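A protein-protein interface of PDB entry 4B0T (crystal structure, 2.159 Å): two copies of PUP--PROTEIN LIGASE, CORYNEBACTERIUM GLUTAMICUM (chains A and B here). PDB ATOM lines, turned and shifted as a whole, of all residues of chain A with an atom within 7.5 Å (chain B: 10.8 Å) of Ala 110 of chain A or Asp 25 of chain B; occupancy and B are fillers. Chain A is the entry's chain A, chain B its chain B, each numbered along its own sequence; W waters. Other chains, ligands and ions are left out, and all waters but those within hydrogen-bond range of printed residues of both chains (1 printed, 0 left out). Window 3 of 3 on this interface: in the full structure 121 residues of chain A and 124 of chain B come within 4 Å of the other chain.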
ATOM      1  N   GLU A 101       7.637 -14.989  27.576  1.00  0.00           N
ATOM      2  CA  GLU A 101       7.391 -13.764  26.809  1.00  0.00           C
ATOM      3  C   GLU A 101       8.513 -12.741  26.985  1.00  0.00           C
ATOM      4  O   GLU A 101       8.886 -12.040  26.036  1.00  0.00           O
ATOM      5  CB  GLU A 101       6.051 -13.126  27.196  1.00  0.00           C
ATOM      6  CG  GLU A 101       4.848 -14.000  26.901  1.00  0.00           C
ATOM      7  CD  GLU A 101       3.510 -13.321  27.186  1.00  0.00           C
ATOM      8  OE1 GLU A 101       3.510 -12.158  27.669  1.00  0.00           O
ATOM      9  OE2 GLU A 101       2.456 -13.963  26.922  1.00  0.00           O
ATOM     10  N   LEU A 104      11.781 -13.829  25.291  1.00  0.00           N
ATOM     11  CA  LEU A 104      11.588 -13.590  23.868  1.00  0.00           C
ATOM     12  C   LEU A 104      11.710 -12.110  23.559  1.00  0.00           C
ATOM     13  O   LEU A 104      12.352 -11.727  22.587  1.00  0.00           O
ATOM     14  CB  LEU A 104      10.229 -14.099  23.400  1.00  0.00           C
ATOM     15  CG  LEU A 104      10.081 -15.615  23.399  1.00  0.00           C
ATOM     16  CD1 LEU A 104       8.764 -16.011  22.760  1.00  0.00           C
ATOM     17  CD2 LEU A 104      11.244 -16.251  22.671  1.00  0.00           C
ATOM     18  N   ALA A 105      11.087 -11.276  24.381  1.00  0.00           N
ATOM     19  CA  ALA A 105      11.129  -9.839  24.142  1.00  0.00           C
ATOM     20  C   ALA A 105      12.547  -9.296  24.275  1.00  0.00           C
ATOM     21  O   ALA A 105      12.897  -8.315  23.622  1.00  0.00           O
ATOM     22  CB  ALA A 105      10.191  -9.104  25.076  1.00  0.00           C
ATOM     23  N   LYS A 106      13.358  -9.929  25.118  1.00  0.00           N
ATOM     24  CA  LYS A 106      14.753  -9.525  25.266  1.00  0.00           C
ATOM     25  C   LYS A 106      15.476  -9.770  23.954  1.00  0.00           C
ATOM     26  O   LYS A 106      16.324  -8.983  23.537  1.00  0.00           O
ATOM     27  CB  LYS A 106      15.427 -10.279  26.410  1.00  0.00           C
ATOM     28  CG  LYS A 106      15.480  -9.485  27.703  1.00  0.00           C
ATOM     29  CD  LYS A 106      15.679 -10.386  28.915  1.00  0.00           C
ATOM     30  CE  LYS A 106      14.512 -11.356  29.076  1.00  0.00           C
ATOM     31  NZ  LYS A 106      14.507 -12.054  30.396  1.00  0.00           N
ATOM     32  N   GLU A 107      15.147 -10.887  23.321  1.00  0.00           N
ATOM     33  CA  GLU A 107      15.482 -11.114  21.926  1.00  0.00           C
ATOM     34  C   GLU A 107      14.538 -10.273  21.080  1.00  0.00           C
ATOM     35  O   GLU A 107      13.523  -9.792  21.574  1.00  0.00           O
ATOM     36  CB  GLU A 107      15.382 -12.597  21.580  1.00  0.00           C
ATOM     37  CG  GLU A 107      16.062 -13.489  22.611  1.00  0.00           C
ATOM     38  CD  GLU A 107      16.527 -14.813  22.039  1.00  0.00           C
ATOM     39  OE1 GLU A 107      16.280 -15.061  20.840  1.00  0.00           O
ATOM     40  OE2 GLU A 107      17.147 -15.603  22.787  1.00  0.00           O
ATOM     41  N   ASP A 108      14.893 -10.046  19.824  1.00  0.00           N
ATOM     42  CA  ASP A 108      14.044  -9.272  18.924  1.00  0.00           C
ATOM     43  C   ASP A 108      12.583  -9.742  18.944  1.00  0.00           C
ATOM     44  O   ASP A 108      11.663  -8.926  18.955  1.00  0.00           O
ATOM     45  CB  ASP A 108      14.600  -9.340  17.497  1.00  0.00           C
ATOM     46  CG  ASP A 108      13.746  -8.582  16.496  1.00  0.00           C
ATOM     47  OD1 ASP A 108      12.705  -9.127  16.067  1.00  0.00           O
ATOM     48  OD2 ASP A 108      14.123  -7.446  16.129  1.00  0.00           O
ATOM     49  N   ILE A 109      12.381 -11.057  18.956  1.00  0.00           N
ATOM     50  CA  ILE A 109      11.046 -11.647  18.814  1.00  0.00           C
ATOM     51  C   ILE A 109      10.042 -11.315  19.930  1.00  0.00           C
ATOM     52  O   ILE A 109      10.352 -11.402  21.117  1.00  0.00           O
ATOM     53  CB  ILE A 109      11.123 -13.179  18.618  1.00  0.00           C
ATOM     54  CG1 ILE A 109       9.819 -13.841  19.070  1.00  0.00           C
ATOM     55  CG2 ILE A 109      12.314 -13.758  19.362  1.00  0.00           C
ATOM     56  CD1 ILE A 109       9.751 -15.337  18.786  1.00  0.00           C
ATOM     57  N   ALA A 110       8.832 -10.940  19.532  1.00  0.00           N
ATOM     58  CA  ALA A 110       7.798 -10.581  20.492  1.00  0.00           C
ATOM     59  C   ALA A 110       6.474 -11.245  20.139  1.00  0.00           C
ATOM     60  O   ALA A 110       6.231 -11.591  18.983  1.00  0.00           O
ATOM     61  CB  ALA A 110       7.639  -9.070  20.564  1.00  0.00           C
ATOM     62  N   GLY A 111       5.622 -11.428  21.141  1.00  0.00           N
ATOM     63  CA  GLY A 111       4.357 -12.112  20.942  1.00  0.00           C
ATOM     64  C   GLY A 111       3.797 -12.628  22.251  1.00  0.00           C
ATOM     65  O   GLY A 111       4.388 -12.421  23.308  1.00  0.00           O
ATOM     66  N   GLN A 112       2.655 -13.300  22.192  1.00  0.00           N
ATOM     67  CA  GLN A 112       2.004 -13.751  23.420  1.00  0.00           C
ATOM     68  C   GLN A 112       1.950 -15.263  23.600  1.00  0.00           C
ATOM     69  O   GLN A 112       1.663 -16.000  22.662  1.00  0.00           O
ATOM     70  CB  GLN A 112       0.600 -13.173  23.501  1.00  0.00           C
ATOM     71  CG  GLN A 112       0.589 -11.681  23.749  1.00  0.00           C
ATOM     72  CD  GLN A 112      -0.813 -11.162  23.914  1.00  0.00           C
ATOM     73  OE1 GLN A 112      -1.190 -10.676  24.983  1.00  0.00           O
ATOM     74  NE2 GLN A 112      -1.604 -11.276  22.856  1.00  0.00           N
ATOM     75  N   THR B  22      -0.219 -22.401  23.558  1.00  0.00           N
ATOM     76  CA  THR B  22      -0.110 -21.862  22.207  1.00  0.00           C
ATOM     77  C   THR B  22       0.530 -20.482  22.178  1.00  0.00           C
ATOM     78  O   THR B  22       0.427 -19.708  23.140  1.00  0.00           O
ATOM     79  CB  THR B  22      -1.474 -21.811  21.497  1.00  0.00           C
ATOM     80  OG1 THR B  22      -2.329 -20.876  22.161  1.00  0.00           O
ATOM     81  CG2 THR B  22      -2.129 -23.188  21.508  1.00  0.00           C
ATOM     82  N   PHE B  23       1.193 -20.184  21.066  1.00  0.00           N
ATOM     83  CA  PHE B  23       1.906 -18.932  20.913  1.00  0.00           C
ATOM     84  C   PHE B  23       1.351 -18.125  19.735  1.00  0.00           C
ATOM     85  O   PHE B  23       1.208 -18.645  18.635  1.00  0.00           O
ATOM     86  CB  PHE B  23       3.403 -19.205  20.730  1.00  0.00           C
ATOM     87  CG  PHE B  23       4.245 -17.958  20.649  1.00  0.00           C
ATOM     88  CD1 PHE B  23       4.444 -17.164  21.772  1.00  0.00           C
ATOM     89  CD2 PHE B  23       4.845 -17.582  19.450  1.00  0.00           C
ATOM     90  CE1 PHE B  23       5.218 -16.012  21.708  1.00  0.00           C
ATOM     91  CE2 PHE B  23       5.625 -16.425  19.372  1.00  0.00           C
ATOM     92  CZ  PHE B  23       5.814 -15.640  20.506  1.00  0.00           C
ATOM     93  N   VAL B  24       1.033 -16.857  19.981  1.00  0.00           N
ATOM     94  CA  VAL B  24       0.555 -15.948  18.935  1.00  0.00           C
ATOM     95  C   VAL B  24       1.601 -14.887  18.614  1.00  0.00           C
ATOM     96  O   VAL B  24       2.058 -14.164  19.504  1.00  0.00           O
ATOM     97  CB  VAL B  24      -0.734 -15.225  19.348  1.00  0.00           C
ATOM     98  CG1 VAL B  24      -1.169 -14.267  18.255  1.00  0.00           C
ATOM     99  CG2 VAL B  24      -1.827 -16.229  19.656  1.00  0.00           C
ATOM    100  N   ASP B  25       1.973 -14.797  17.341  1.00  0.00           N
ATOM    101  CA  ASP B  25       3.014 -13.871  16.900  1.00  0.00           C
ATOM    102  C   ASP B  25       2.523 -12.432  16.860  1.00  0.00           C
ATOM    103  O   ASP B  25       3.313 -11.512  16.652  1.00  0.00           O
ATOM    104  CB  ASP B  25       3.557 -14.273  15.525  1.00  0.00           C
ATOM    105  CG  ASP B  25       4.469 -15.490  15.586  1.00  0.00           C
ATOM    106  OD1 ASP B  25       4.109 -16.479  16.264  1.00  0.00           O
ATOM    107  OD2 ASP B  25       5.548 -15.455  14.953  1.00  0.00           O
ATOM    108  N   LEU B  31       7.911 -18.965  16.247  1.00  0.00           N
ATOM    109  CA  LEU B  31       8.852 -20.075  16.175  1.00  0.00           C
ATOM    110  C   LEU B  31       8.111 -21.394  16.201  1.00  0.00           C
ATOM    111  O   LEU B  31       6.889 -21.426  16.348  1.00  0.00           O
ATOM    112  CB  LEU B  31       9.815 -20.038  17.357  1.00  0.00           C
ATOM    113  CG  LEU B  31      10.612 -18.754  17.549  1.00  0.00           C
ATOM    114  CD1 LEU B  31      11.515 -18.879  18.763  1.00  0.00           C
ATOM    115  CD2 LEU B  31      11.417 -18.445  16.297  1.00  0.00           C
ATOM    116  N   ARG B  32       8.856 -22.484  16.060  1.00  0.00           N
ATOM    117  CA  ARG B  32       8.297 -23.808  16.272  1.00  0.00           C
ATOM    118  C   ARG B  32       7.760 -23.880  17.695  1.00  0.00           C
ATOM    119  O   ARG B  32       8.441 -23.465  18.634  1.00  0.00           O
ATOM    120  CB  ARG B  32       9.373 -24.873  16.082  1.00  0.00           C
ATOM    121  CG  ARG B  32       9.867 -25.009  14.663  1.00  0.00           C
ATOM    122  CD  ARG B  32      11.092 -25.894  14.608  1.00  0.00           C
ATOM    123  NE  ARG B  32      11.439 -26.257  13.240  1.00  0.00           N
ATOM    124  CZ  ARG B  32      12.546 -26.910  12.897  1.00  0.00           C
ATOM    125  NH1 ARG B  32      13.420 -27.268  13.829  1.00  0.00           N
ATOM    126  NH2 ARG B  32      12.782 -27.201  11.624  1.00  0.00           N
ATOM    127  N   PRO B  33       6.535 -24.403  17.863  1.00  0.00           N
ATOM    128  CA  PRO B  33       5.976 -24.546  19.209  1.00  0.00           C
ATOM    129  C   PRO B  33       6.900 -25.382  20.084  1.00  0.00           C
ATOM    130  O   PRO B  33       6.915 -25.198  21.301  1.00  0.00           O
ATOM    131  CB  PRO B  33       4.645 -25.270  18.968  1.00  0.00           C
ATOM    132  CG  PRO B  33       4.766 -25.876  17.623  1.00  0.00           C
ATOM    133  CD  PRO B  33       5.634 -24.944  16.835  1.00  0.00           C
ATOM    134  N   GLU B  35      10.079 -25.075  20.070  1.00  0.00           N
ATOM    135  CA  GLU B  35      11.020 -24.081  20.553  1.00  0.00           C
ATOM    136  C   GLU B  35      10.407 -23.188  21.628  1.00  0.00           C
ATOM    137  O   GLU B  35      11.118 -22.658  22.484  1.00  0.00           O
ATOM    138  CB  GLU B  35      11.532 -23.232  19.392  1.00  0.00           C
ATOM    139  CG  GLU B  35      12.290 -21.983  19.826  1.00  0.00           C
ATOM    140  CD  GLU B  35      13.395 -22.274  20.840  1.00  0.00           C
ATOM    141  OE1 GLU B  35      13.560 -23.454  21.221  1.00  0.00           O
ATOM    142  OE2 GLU B  35      14.094 -21.320  21.256  1.00  0.00           O
ATOM    143  N   ILE B  36       9.088 -23.011  21.583  1.00  0.00           N
ATOM    144  CA  ILE B  36       8.422 -22.181  22.583  1.00  0.00           C
ATOM    145  C   ILE B  36       8.316 -22.922  23.919  1.00  0.00           C
ATOM    146  O   ILE B  36       8.566 -22.349  24.982  1.00  0.00           O
ATOM    147  CB  ILE B  36       7.029 -21.699  22.114  1.00  0.00           C
ATOM    148  CG1 ILE B  36       7.181 -20.678  20.986  1.00  0.00           C
ATOM    149  CG2 ILE B  36       6.247 -21.085  23.277  1.00  0.00           C
ATOM    150  CD1 ILE B  36       7.982 -19.446  21.383  1.00  0.00           C
ATOM    151  N   ARG B  39      11.882 -23.278  25.595  1.00  0.00           N
ATOM    152  CA  ARG B  39      12.287 -22.067  26.297  1.00  0.00           C
ATOM    153  C   ARG B  39      11.480 -21.826  27.576  1.00  0.00           C
ATOM    154  O   ARG B  39      12.003 -21.345  28.582  1.00  0.00           O
ATOM    155  CB  ARG B  39      12.151 -20.860  25.377  1.00  0.00           C
ATOM    156  CG  ARG B  39      12.343 -19.545  26.092  1.00  0.00           C
ATOM    157  CD  ARG B  39      12.264 -18.390  25.114  1.00  0.00           C
ATOM    158  NE  ARG B  39      13.285 -18.501  24.078  1.00  0.00           N
ATOM    159  CZ  ARG B  39      13.985 -17.475  23.608  1.00  0.00           C
ATOM    160  NH1 ARG B  39      13.773 -16.254  24.081  1.00  0.00           N
ATOM    161  NH2 ARG B  39      14.897 -17.674  22.665  1.00  0.00           N
HETATM  162  O   HOH W   1       0.359 -11.509  20.237  1.00  0.00           O
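The backbone NH (N) of Leu 104 of chain A sits close to the guanidinium group (NH1) of Arg 39 of chain B. N of Val 24 of chain B is in hydrogen-bond range of O of Gln 112 of chain A. OE2 of Glu 107 of chain A lies within salt-bridge range of NH2 of Arg 39 of chain B, at 3.1 Å.
The backbone carbonyl oxygen (O) of Leu 104 of chain A sits close to the backbone carbonyl oxygen (O) of Ile 109 of chain A, at 2.5 Å. The side-chain carboxylate of Glu 35 of chain B is in salt-bridge range of the guanidinium group of Arg 39 of chain B, 3.99 Å away.
Leu 104 of chain A touches Phe 23 of chain B. Leu 104 of chain A touches Ile 36 of chain B. Leu 31 of chain B touches Ile 109 of chain A. O of Asp 25 of chain B touches O of Ala 110 of chain A, at 3.7 Å. Gly 111 of chain A touches Phe 23 of chain B. Gly 111 of chain A touches Val 24 of chain B. Gln 112 of chain A touches Thr 22 of chain B (O to O, 3.9 Å). Gln 112 of chain A touches Phe 23 of chain B (O to CD1, 3.1 Å).
Of chain B, only Asp 25 comes within 4 Å of Ala 110 of chain A. Of chain A, only Ala 110 (3.7 Å) comes within 4 Å of Asp 25 of chain B. No residue of chain B comes within 4 Å of Ala 105 of chain A. Printed residues of chain B within 4 Å of Ile 109 of chain A: Leu 31. Gly 111 of chain A touches two residues of chain B. Of the printed residues of chain A, Leu 31 of chain B touches Ile 109. Of the printed residues of chain A, Thr 22 of chain B touches Gln 112 (3.9 Å). Printed residues of chain A within 4 Å of Arg 39 of chain B: Leu 104 and Glu 107. Printed residues of chain A within 4 Å of Phe 23 of chain B: Leu 104 (3.7 Å), Gly 111 (3.7 Å) and Gln 112 (3.1 Å). Of the printed residues of chain B, Leu 104 of chain A touches Phe 23, Ile 36 and Arg 39.
Of the 10 printed residues of chain A, 6 touch a printed residue of chain B. Hydrophobic or aromatic side chains of chain A within 4 Å of the printed part of chain B: Leu 104 and Ile 109. Among the printed residues, Asp or Glu carboxylates within 4 Å of a Lys or Arg side-chain nitrogen of the other chain: Glu 107 of chain A with Arg 39 of chain B (3.1 Å).
No position is printed for both chains. Of the 11 pairs that touch across the chains among the printed residues, none has its exchanged pair printed and touching as well.
Water W1 lies within hydrogen-bond range of the backbone carbonyl oxygen of Val 24 of chain B and the side-chain amide nitrogen of Gln 112 of chain A.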
